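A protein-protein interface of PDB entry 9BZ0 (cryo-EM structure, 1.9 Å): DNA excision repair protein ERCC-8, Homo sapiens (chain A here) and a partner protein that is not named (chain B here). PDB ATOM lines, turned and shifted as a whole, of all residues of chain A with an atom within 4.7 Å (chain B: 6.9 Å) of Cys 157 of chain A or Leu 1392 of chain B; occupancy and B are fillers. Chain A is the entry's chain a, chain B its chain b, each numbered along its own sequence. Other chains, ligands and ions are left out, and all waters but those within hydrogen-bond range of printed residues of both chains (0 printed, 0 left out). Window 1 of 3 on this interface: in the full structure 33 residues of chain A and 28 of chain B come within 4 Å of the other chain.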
ATOM      1  N   TYR A 108       4.568   5.129  14.911  1.00  0.00           N
ATOM      2  CA  TYR A 108       4.041   4.920  13.576  1.00  0.00           C
ATOM      3  C   TYR A 108       5.187   4.550  12.642  1.00  0.00           C
ATOM      4  O   TYR A 108       6.216   5.231  12.638  1.00  0.00           O
ATOM      5  CB  TYR A 108       3.326   6.178  13.100  1.00  0.00           C
ATOM      6  CG  TYR A 108       2.613   6.076  11.781  1.00  0.00           C
ATOM      7  CD1 TYR A 108       1.647   5.124  11.563  1.00  0.00           C
ATOM      8  CD2 TYR A 108       2.889   6.959  10.764  1.00  0.00           C
ATOM      9  CE1 TYR A 108       1.000   5.046  10.368  1.00  0.00           C
ATOM     10  CE2 TYR A 108       2.243   6.889   9.574  1.00  0.00           C
ATOM     11  CZ  TYR A 108       1.305   5.930   9.376  1.00  0.00           C
ATOM     12  OH  TYR A 108       0.658   5.873   8.172  1.00  0.00           O
ATOM     13  N   MET A 114       3.498  10.525  14.858  1.00  0.00           N
ATOM     14  CA  MET A 114       2.430   9.855  15.573  1.00  0.00           C
ATOM     15  C   MET A 114       2.985   8.614  16.247  1.00  0.00           C
ATOM     16  O   MET A 114       3.910   7.984  15.741  1.00  0.00           O
ATOM     17  CB  MET A 114       1.316   9.516  14.591  1.00  0.00           C
ATOM     18  CG  MET A 114       0.309   8.541  15.054  1.00  0.00           C
ATOM     19  SD  MET A 114      -0.788   8.137  13.695  1.00  0.00           S
ATOM     20  CE  MET A 114      -0.879   6.369  13.897  1.00  0.00           C
ATOM     21  N   LYS A 155      -0.416   0.007   2.372  1.00  0.00           N
ATOM     22  CA  LYS A 155      -1.757  -0.074   1.814  1.00  0.00           C
ATOM     23  C   LYS A 155      -2.819   0.136   2.880  1.00  0.00           C
ATOM     24  O   LYS A 155      -3.867   0.728   2.610  1.00  0.00           O
ATOM     25  CB  LYS A 155      -1.953  -1.421   1.123  1.00  0.00           C
ATOM     26  CG  LYS A 155      -1.116  -1.598  -0.133  1.00  0.00           C
ATOM     27  CD  LYS A 155      -1.375  -2.947  -0.786  1.00  0.00           C
ATOM     28  CE  LYS A 155      -0.518  -3.130  -2.028  1.00  0.00           C
ATOM     29  NZ  LYS A 155      -0.734  -4.454  -2.672  1.00  0.00           N
ATOM     30  N   HIS A 156      -2.560  -0.331   4.095  1.00  0.00           N
ATOM     31  CA  HIS A 156      -3.515  -0.281   5.186  1.00  0.00           C
ATOM     32  C   HIS A 156      -2.820   0.142   6.464  1.00  0.00           C
ATOM     33  O   HIS A 156      -1.606   0.003   6.612  1.00  0.00           O
ATOM     34  CB  HIS A 156      -4.159  -1.646   5.424  1.00  0.00           C
ATOM     35  CG  HIS A 156      -3.242  -2.622   6.097  1.00  0.00           C
ATOM     36  ND1 HIS A 156      -3.061  -2.660   7.461  1.00  0.00           N
ATOM     37  CD2 HIS A 156      -2.465  -3.606   5.591  1.00  0.00           C
ATOM     38  CE1 HIS A 156      -2.194  -3.607   7.763  1.00  0.00           C
ATOM     39  NE2 HIS A 156      -1.822  -4.201   6.647  1.00  0.00           N
ATOM     40  N   CYS A 157      -3.602   0.681   7.385  1.00  0.00           N
ATOM     41  CA  CYS A 157      -3.106   1.142   8.674  1.00  0.00           C
ATOM     42  C   CYS A 157      -3.872   0.429   9.786  1.00  0.00           C
ATOM     43  O   CYS A 157      -4.639   1.053  10.510  1.00  0.00           O
ATOM     44  CB  CYS A 157      -3.231   2.644   8.782  1.00  0.00           C
ATOM     45  SG  CYS A 157      -2.330   3.353  10.159  1.00  0.00           S
ATOM     46  N   LEU A 158      -3.648  -0.869   9.936  1.00  0.00           N
ATOM     47  CA  LEU A 158      -4.384  -1.683  10.894  1.00  0.00           C
ATOM     48  C   LEU A 158      -3.519  -1.949  12.110  1.00  0.00           C
ATOM     49  O   LEU A 158      -2.366  -2.360  11.982  1.00  0.00           O
ATOM     50  CB  LEU A 158      -4.831  -3.002  10.277  1.00  0.00           C
ATOM     51  CG  LEU A 158      -5.975  -2.979   9.283  1.00  0.00           C
ATOM     52  CD1 LEU A 158      -6.086  -4.314   8.632  1.00  0.00           C
ATOM     53  CD2 LEU A 158      -7.256  -2.631   9.973  1.00  0.00           C
ATOM     54  N   VAL A 159      -4.086  -1.721  13.284  1.00  0.00           N
ATOM     55  CA  VAL A 159      -3.512  -2.142  14.553  1.00  0.00           C
ATOM     56  C   VAL A 159      -4.167  -3.442  14.991  1.00  0.00           C
ATOM     57  O   VAL A 159      -5.382  -3.494  15.200  1.00  0.00           O
ATOM     58  CB  VAL A 159      -3.687  -1.058  15.621  1.00  0.00           C
ATOM     59  CG1 VAL A 159      -2.924  -1.418  16.846  1.00  0.00           C
ATOM     60  CG2 VAL A 159      -3.230   0.266  15.100  1.00  0.00           C
ATOM     61  N   CYS A 171      -7.993  -2.727  14.614  1.00  0.00           N
ATOM     62  CA  CYS A 171      -8.462  -1.353  14.538  1.00  0.00           C
ATOM     63  C   CYS A 171      -7.882  -0.682  13.305  1.00  0.00           C
ATOM     64  O   CYS A 171      -6.665  -0.678  13.112  1.00  0.00           O
ATOM     65  CB  CYS A 171      -8.078  -0.573  15.789  1.00  0.00           C
ATOM     66  SG  CYS A 171      -8.709  -1.270  17.302  1.00  0.00           S
ATOM     67  N   ASP A 172      -8.751  -0.115  12.481  1.00  0.00           N
ATOM     68  CA  ASP A 172      -8.347   0.619  11.291  1.00  0.00           C
ATOM     69  C   ASP A 172      -8.291   2.100  11.628  1.00  0.00           C
ATOM     70  O   ASP A 172      -9.327   2.743  11.804  1.00  0.00           O
ATOM     71  CB  ASP A 172      -9.326   0.337  10.157  1.00  0.00           C
ATOM     72  CG  ASP A 172      -9.025   1.125   8.910  1.00  0.00           C
ATOM     73  OD1 ASP A 172      -7.913   1.675   8.792  1.00  0.00           O
ATOM     74  OD2 ASP A 172      -9.910   1.189   8.035  1.00  0.00           O
ATOM     75  N   LEU A 173      -7.080   2.641  11.708  1.00  0.00           N
ATOM     76  CA  LEU A 173      -6.912   4.039  12.066  1.00  0.00           C
ATOM     77  C   LEU A 173      -7.434   4.975  10.996  1.00  0.00           C
ATOM     78  O   LEU A 173      -7.813   6.106  11.300  1.00  0.00           O
ATOM     79  CB  LEU A 173      -5.451   4.339  12.358  1.00  0.00           C
ATOM     80  CG  LEU A 173      -4.804   3.497  13.442  1.00  0.00           C
ATOM     81  CD1 LEU A 173      -3.465   4.057  13.761  1.00  0.00           C
ATOM     82  CD2 LEU A 173      -5.666   3.478  14.672  1.00  0.00           C
ATOM     83  N   LYS A 174      -7.451   4.537   9.745  1.00  0.00           N
ATOM     84  CA  LYS A 174      -7.952   5.383   8.673  1.00  0.00           C
ATOM     85  C   LYS A 174      -9.454   5.605   8.793  1.00  0.00           C
ATOM     86  O   LYS A 174      -9.926   6.745   8.772  1.00  0.00           O
ATOM     87  CB  LYS A 174      -7.594   4.774   7.325  1.00  0.00           C
ATOM     88  CG  LYS A 174      -7.720   5.732   6.173  1.00  0.00           C
ATOM     89  CD  LYS A 174      -7.461   5.035   4.854  1.00  0.00           C
ATOM     90  CE  LYS A 174      -7.574   6.001   3.687  1.00  0.00           C
ATOM     91  NZ  LYS A 174      -7.437   5.310   2.374  1.00  0.00           N
ATOM     92  N   LEU B1387       0.615   6.835   3.968  1.00  0.00           N
ATOM     93  CA  LEU B1387      -0.021   8.027   4.504  1.00  0.00           C
ATOM     94  C   LEU B1387       0.921   8.741   5.454  1.00  0.00           C
ATOM     95  O   LEU B1387       1.515   8.126   6.339  1.00  0.00           O
ATOM     96  CB  LEU B1387      -1.317   7.665   5.217  1.00  0.00           C
ATOM     97  CG  LEU B1387      -2.384   7.015   4.340  1.00  0.00           C
ATOM     98  CD1 LEU B1387      -3.612   6.667   5.160  1.00  0.00           C
ATOM     99  CD2 LEU B1387      -2.750   7.929   3.182  1.00  0.00           C
ATOM    100  N   ALA B1388       1.055  10.041   5.263  1.00  0.00           N
ATOM    101  CA  ALA B1388       1.780  10.862   6.207  1.00  0.00           C
ATOM    102  C   ALA B1388       0.980  10.999   7.485  1.00  0.00           C
ATOM    103  O   ALA B1388      -0.251  11.018   7.474  1.00  0.00           O
ATOM    104  CB  ALA B1388       2.067  12.238   5.616  1.00  0.00           C
ATOM    105  N   SER B1389       1.694  11.065   8.597  1.00  0.00           N
ATOM    106  CA  SER B1389       1.045  11.225   9.885  1.00  0.00           C
ATOM    107  C   SER B1389       0.121  12.428   9.904  1.00  0.00           C
ATOM    108  O   SER B1389      -0.958  12.369  10.490  1.00  0.00           O
ATOM    109  CB  SER B1389       2.089  11.347  10.988  1.00  0.00           C
ATOM    110  OG  SER B1389       1.485  11.634  12.232  1.00  0.00           O
ATOM    111  N   SER B1390       0.549  13.546   9.329  1.00  0.00           N
ATOM    112  CA  SER B1390      -0.258  14.758   9.396  1.00  0.00           C
ATOM    113  C   SER B1390      -1.643  14.602   8.778  1.00  0.00           C
ATOM    114  O   SER B1390      -2.625  15.092   9.344  1.00  0.00           O
ATOM    115  CB  SER B1390       0.486  15.906   8.722  1.00  0.00           C
ATOM    116  OG  SER B1390       1.774  16.070   9.286  1.00  0.00           O
ATOM    117  N   SER B1391      -1.782  13.813   7.721  1.00  0.00           N
ATOM    118  CA  SER B1391      -3.113  13.638   7.153  1.00  0.00           C
ATOM    119  C   SER B1391      -3.952  12.593   7.865  1.00  0.00           C
ATOM    120  O   SER B1391      -5.173  12.761   7.990  1.00  0.00           O
ATOM    121  CB  SER B1391      -2.996  13.264   5.682  1.00  0.00           C
ATOM    122  OG  SER B1391      -2.475  11.962   5.549  1.00  0.00           O
ATOM    123  N   LEU B1392      -3.325  11.559   8.399  1.00  0.00           N
ATOM    124  CA  LEU B1392      -4.045  10.613   9.234  1.00  0.00           C
ATOM    125  C   LEU B1392      -4.535  11.275  10.516  1.00  0.00           C
ATOM    126  O   LEU B1392      -5.686  11.084  10.927  1.00  0.00           O
ATOM    127  CB  LEU B1392      -3.128   9.432   9.525  1.00  0.00           C
ATOM    128  CG  LEU B1392      -3.673   8.162  10.136  1.00  0.00           C
ATOM    129  CD1 LEU B1392      -4.624   7.531   9.159  1.00  0.00           C
ATOM    130  CD2 LEU B1392      -2.528   7.238  10.425  1.00  0.00           C
ATOM    131  N   LEU B1393      -3.677  12.070  11.140  1.00  0.00           N
ATOM    132  CA  LEU B1393      -4.070  12.873  12.286  1.00  0.00           C
ATOM    133  C   LEU B1393      -5.196  13.834  11.952  1.00  0.00           C
ATOM    134  O   LEU B1393      -6.108  14.025  12.762  1.00  0.00           O
ATOM    135  CB  LEU B1393      -2.865  13.642  12.810  1.00  0.00           C
ATOM    136  CG  LEU B1393      -1.808  12.827  13.551  1.00  0.00           C
ATOM    137  CD1 LEU B1393      -0.566  13.665  13.767  1.00  0.00           C
ATOM    138  CD2 LEU B1393      -2.329  12.312  14.861  1.00  0.00           C
ATOM    139  N   ALA B1394      -5.128  14.499  10.798  1.00  0.00           N
ATOM    140  CA  ALA B1394      -6.211  15.394  10.406  1.00  0.00           C
ATOM    141  C   ALA B1394      -7.538  14.668  10.255  1.00  0.00           C
ATOM    142  O   ALA B1394      -8.574  15.167  10.702  1.00  0.00           O
ATOM    143  CB  ALA B1394      -5.855  16.108   9.107  1.00  0.00           C
ATOM    144  N   LYS B1395      -7.533  13.487   9.644  1.00  0.00           N
ATOM    145  CA  LYS B1395      -8.762  12.700   9.560  1.00  0.00           C
ATOM    146  C   LYS B1395      -9.293  12.307  10.932  1.00  0.00           C
ATOM    147  O   LYS B1395     -10.490  12.438  11.200  1.00  0.00           O
ATOM    148  CB  LYS B1395      -8.542  11.457   8.707  1.00  0.00           C
ATOM    149  CG  LYS B1395      -8.371  11.737   7.238  1.00  0.00           C
ATOM    150  CD  LYS B1395      -8.132  10.457   6.467  1.00  0.00           C
ATOM    151  CE  LYS B1395      -7.852  10.739   5.002  1.00  0.00           C
ATOM    152  NZ  LYS B1395      -9.036  11.329   4.317  1.00  0.00           N
ATOM    153  N   MET B1396      -8.423  11.828  11.814  1.00  0.00           N
ATOM    154  CA  MET B1396      -8.844  11.472  13.168  1.00  0.00           C
ATOM    155  C   MET B1396      -9.408  12.662  13.942  1.00  0.00           C
ATOM    156  O   MET B1396     -10.461  12.550  14.584  1.00  0.00           O
ATOM    157  CB  MET B1396      -7.669  10.843  13.911  1.00  0.00           C
ATOM    158  CG  MET B1396      -7.311   9.467  13.379  1.00  0.00           C
ATOM    159  SD  MET B1396      -6.016   8.576  14.251  1.00  0.00           S
ATOM    160  CE  MET B1396      -4.627   9.651  13.960  1.00  0.00           C
ATOM    161  N   ARG B1397      -8.752  13.817  13.866  1.00  0.00           N
ATOM    162  CA  ARG B1397      -9.265  15.016  14.521  1.00  0.00           C
ATOM    163  C   ARG B1397     -10.612  15.444  13.956  1.00  0.00           C
ATOM    164  O   ARG B1397     -11.561  15.684  14.709  1.00  0.00           O
ATOM    165  CB  ARG B1397      -8.251  16.146  14.384  1.00  0.00           C
ATOM    166  CG  ARG B1397      -7.020  15.960  15.230  1.00  0.00           C
ATOM    167  CD  ARG B1397      -5.983  17.013  14.921  1.00  0.00           C
ATOM    168  NE  ARG B1397      -4.800  16.872  15.760  1.00  0.00           N
ATOM    169  CZ  ARG B1397      -4.673  17.401  16.969  1.00  0.00           C
ATOM    170  NH1 ARG B1397      -3.506  17.305  17.598  1.00  0.00           N
ATOM    171  NH2 ARG B1397      -5.695  17.970  17.586  1.00  0.00           N
ATOM    172  N   ARG B1399     -12.761  13.687  12.475  1.00  0.00           N
ATOM    173  CA  ARG B1399     -13.734  12.682  12.865  1.00  0.00           C
ATOM    174  C   ARG B1399     -14.141  12.806  14.324  1.00  0.00           C
ATOM    175  O   ARG B1399     -15.264  12.443  14.680  1.00  0.00           O
ATOM    176  CB  ARG B1399     -13.146  11.301  12.587  1.00  0.00           C
ATOM    177  CG  ARG B1399     -14.030  10.137  12.913  1.00  0.00           C
ATOM    178  CD  ARG B1399     -13.468   8.883  12.288  1.00  0.00           C
ATOM    179  NE  ARG B1399     -12.165   8.550  12.848  1.00  0.00           N
ATOM    180  CZ  ARG B1399     -11.112   8.173  12.139  1.00  0.00           C
ATOM    181  NH1 ARG B1399     -10.035   7.724  12.771  1.00  0.00           N
ATOM    182  NH2 ARG B1399     -11.092   8.279  10.824  1.00  0.00           N
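The side-chain hydroxyl of Tyr 108 of chain A sits at hydrogen-bond distance from the backbone carbonyl oxygen of Leu 1387 of chain B, at 3.0 Å. N of Met 114 of chain A sits close to OG of Ser 1389 of chain B. NH1 of Arg 1399 of chain B lies within hydrogen-bond range of O of Leu 173 of chain A, 3.1 Å away. The backbone carbonyl oxygen (O) of Lys 174 of chain A sits at hydrogen-bond distance from the guanidinium group (NH2) of Arg 1399 of chain B, 2.8 Å away.
N of Tyr 108 of chain A lies within hydrogen-bond range of O of Met 114 of chain A. O of Cys 157 of chain A sits at hydrogen-bond distance from N of Leu 173 of chain A (3.1 Å). The backbone NH (N) of Lys 174 of chain A sits at hydrogen-bond distance from the side-chain carboxylate (OD1) of Asp 172 of chain A (3.1 Å).
SD of Met 114 of chain A touches CD2 of Leu 1392 of chain B, 3.8 Å away. CD2 of Leu 1392 of chain B touches SG of Cys 157 of chain A, 3.9 Å away. Met 1396 of chain B touches Leu 173 of chain A. Leu 1392 of chain B touches Lys 174 of chain A.
Of the printed residues of chain B, Met 114 of chain A touches Ser 1389 (3.2 Å) and Leu 1392 (3.8 Å). His 156 of chain A touches none of the printed residues of chain B. Printed residues of chain B within 4 Å of Cys 157 of chain A: Leu 1392. Of the printed residues of chain B, Lys 174 of chain A touches Leu 1392 and Arg 1399. Of the printed residues of chain A, Ser 1389 of chain B touches Met 114. Printed residues of chain A within 4 Å of Leu 1392 of chain B: Met 114 (3.8 Å), Cys 157 (3.9 Å) and Lys 174 (3.99 Å). Arg 1397 of chain B touches none of the printed residues of chain A. The nearest printed residue of chain A that does not touch Leu 1392 of chain B is Leu 173 of chain A (4.1 Å). The nearest printed residue of chain B that does not touch Lys 174 of chain A is Leu 1387 of chain B (4.2 Å).
Of the 12 printed residues of chain B, 5 touch a printed residue of chain A. Among the printed residues, no Asp or Glu carboxylate lies within 4 Å of a Lys or Arg side-chain nitrogen of the other chain.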
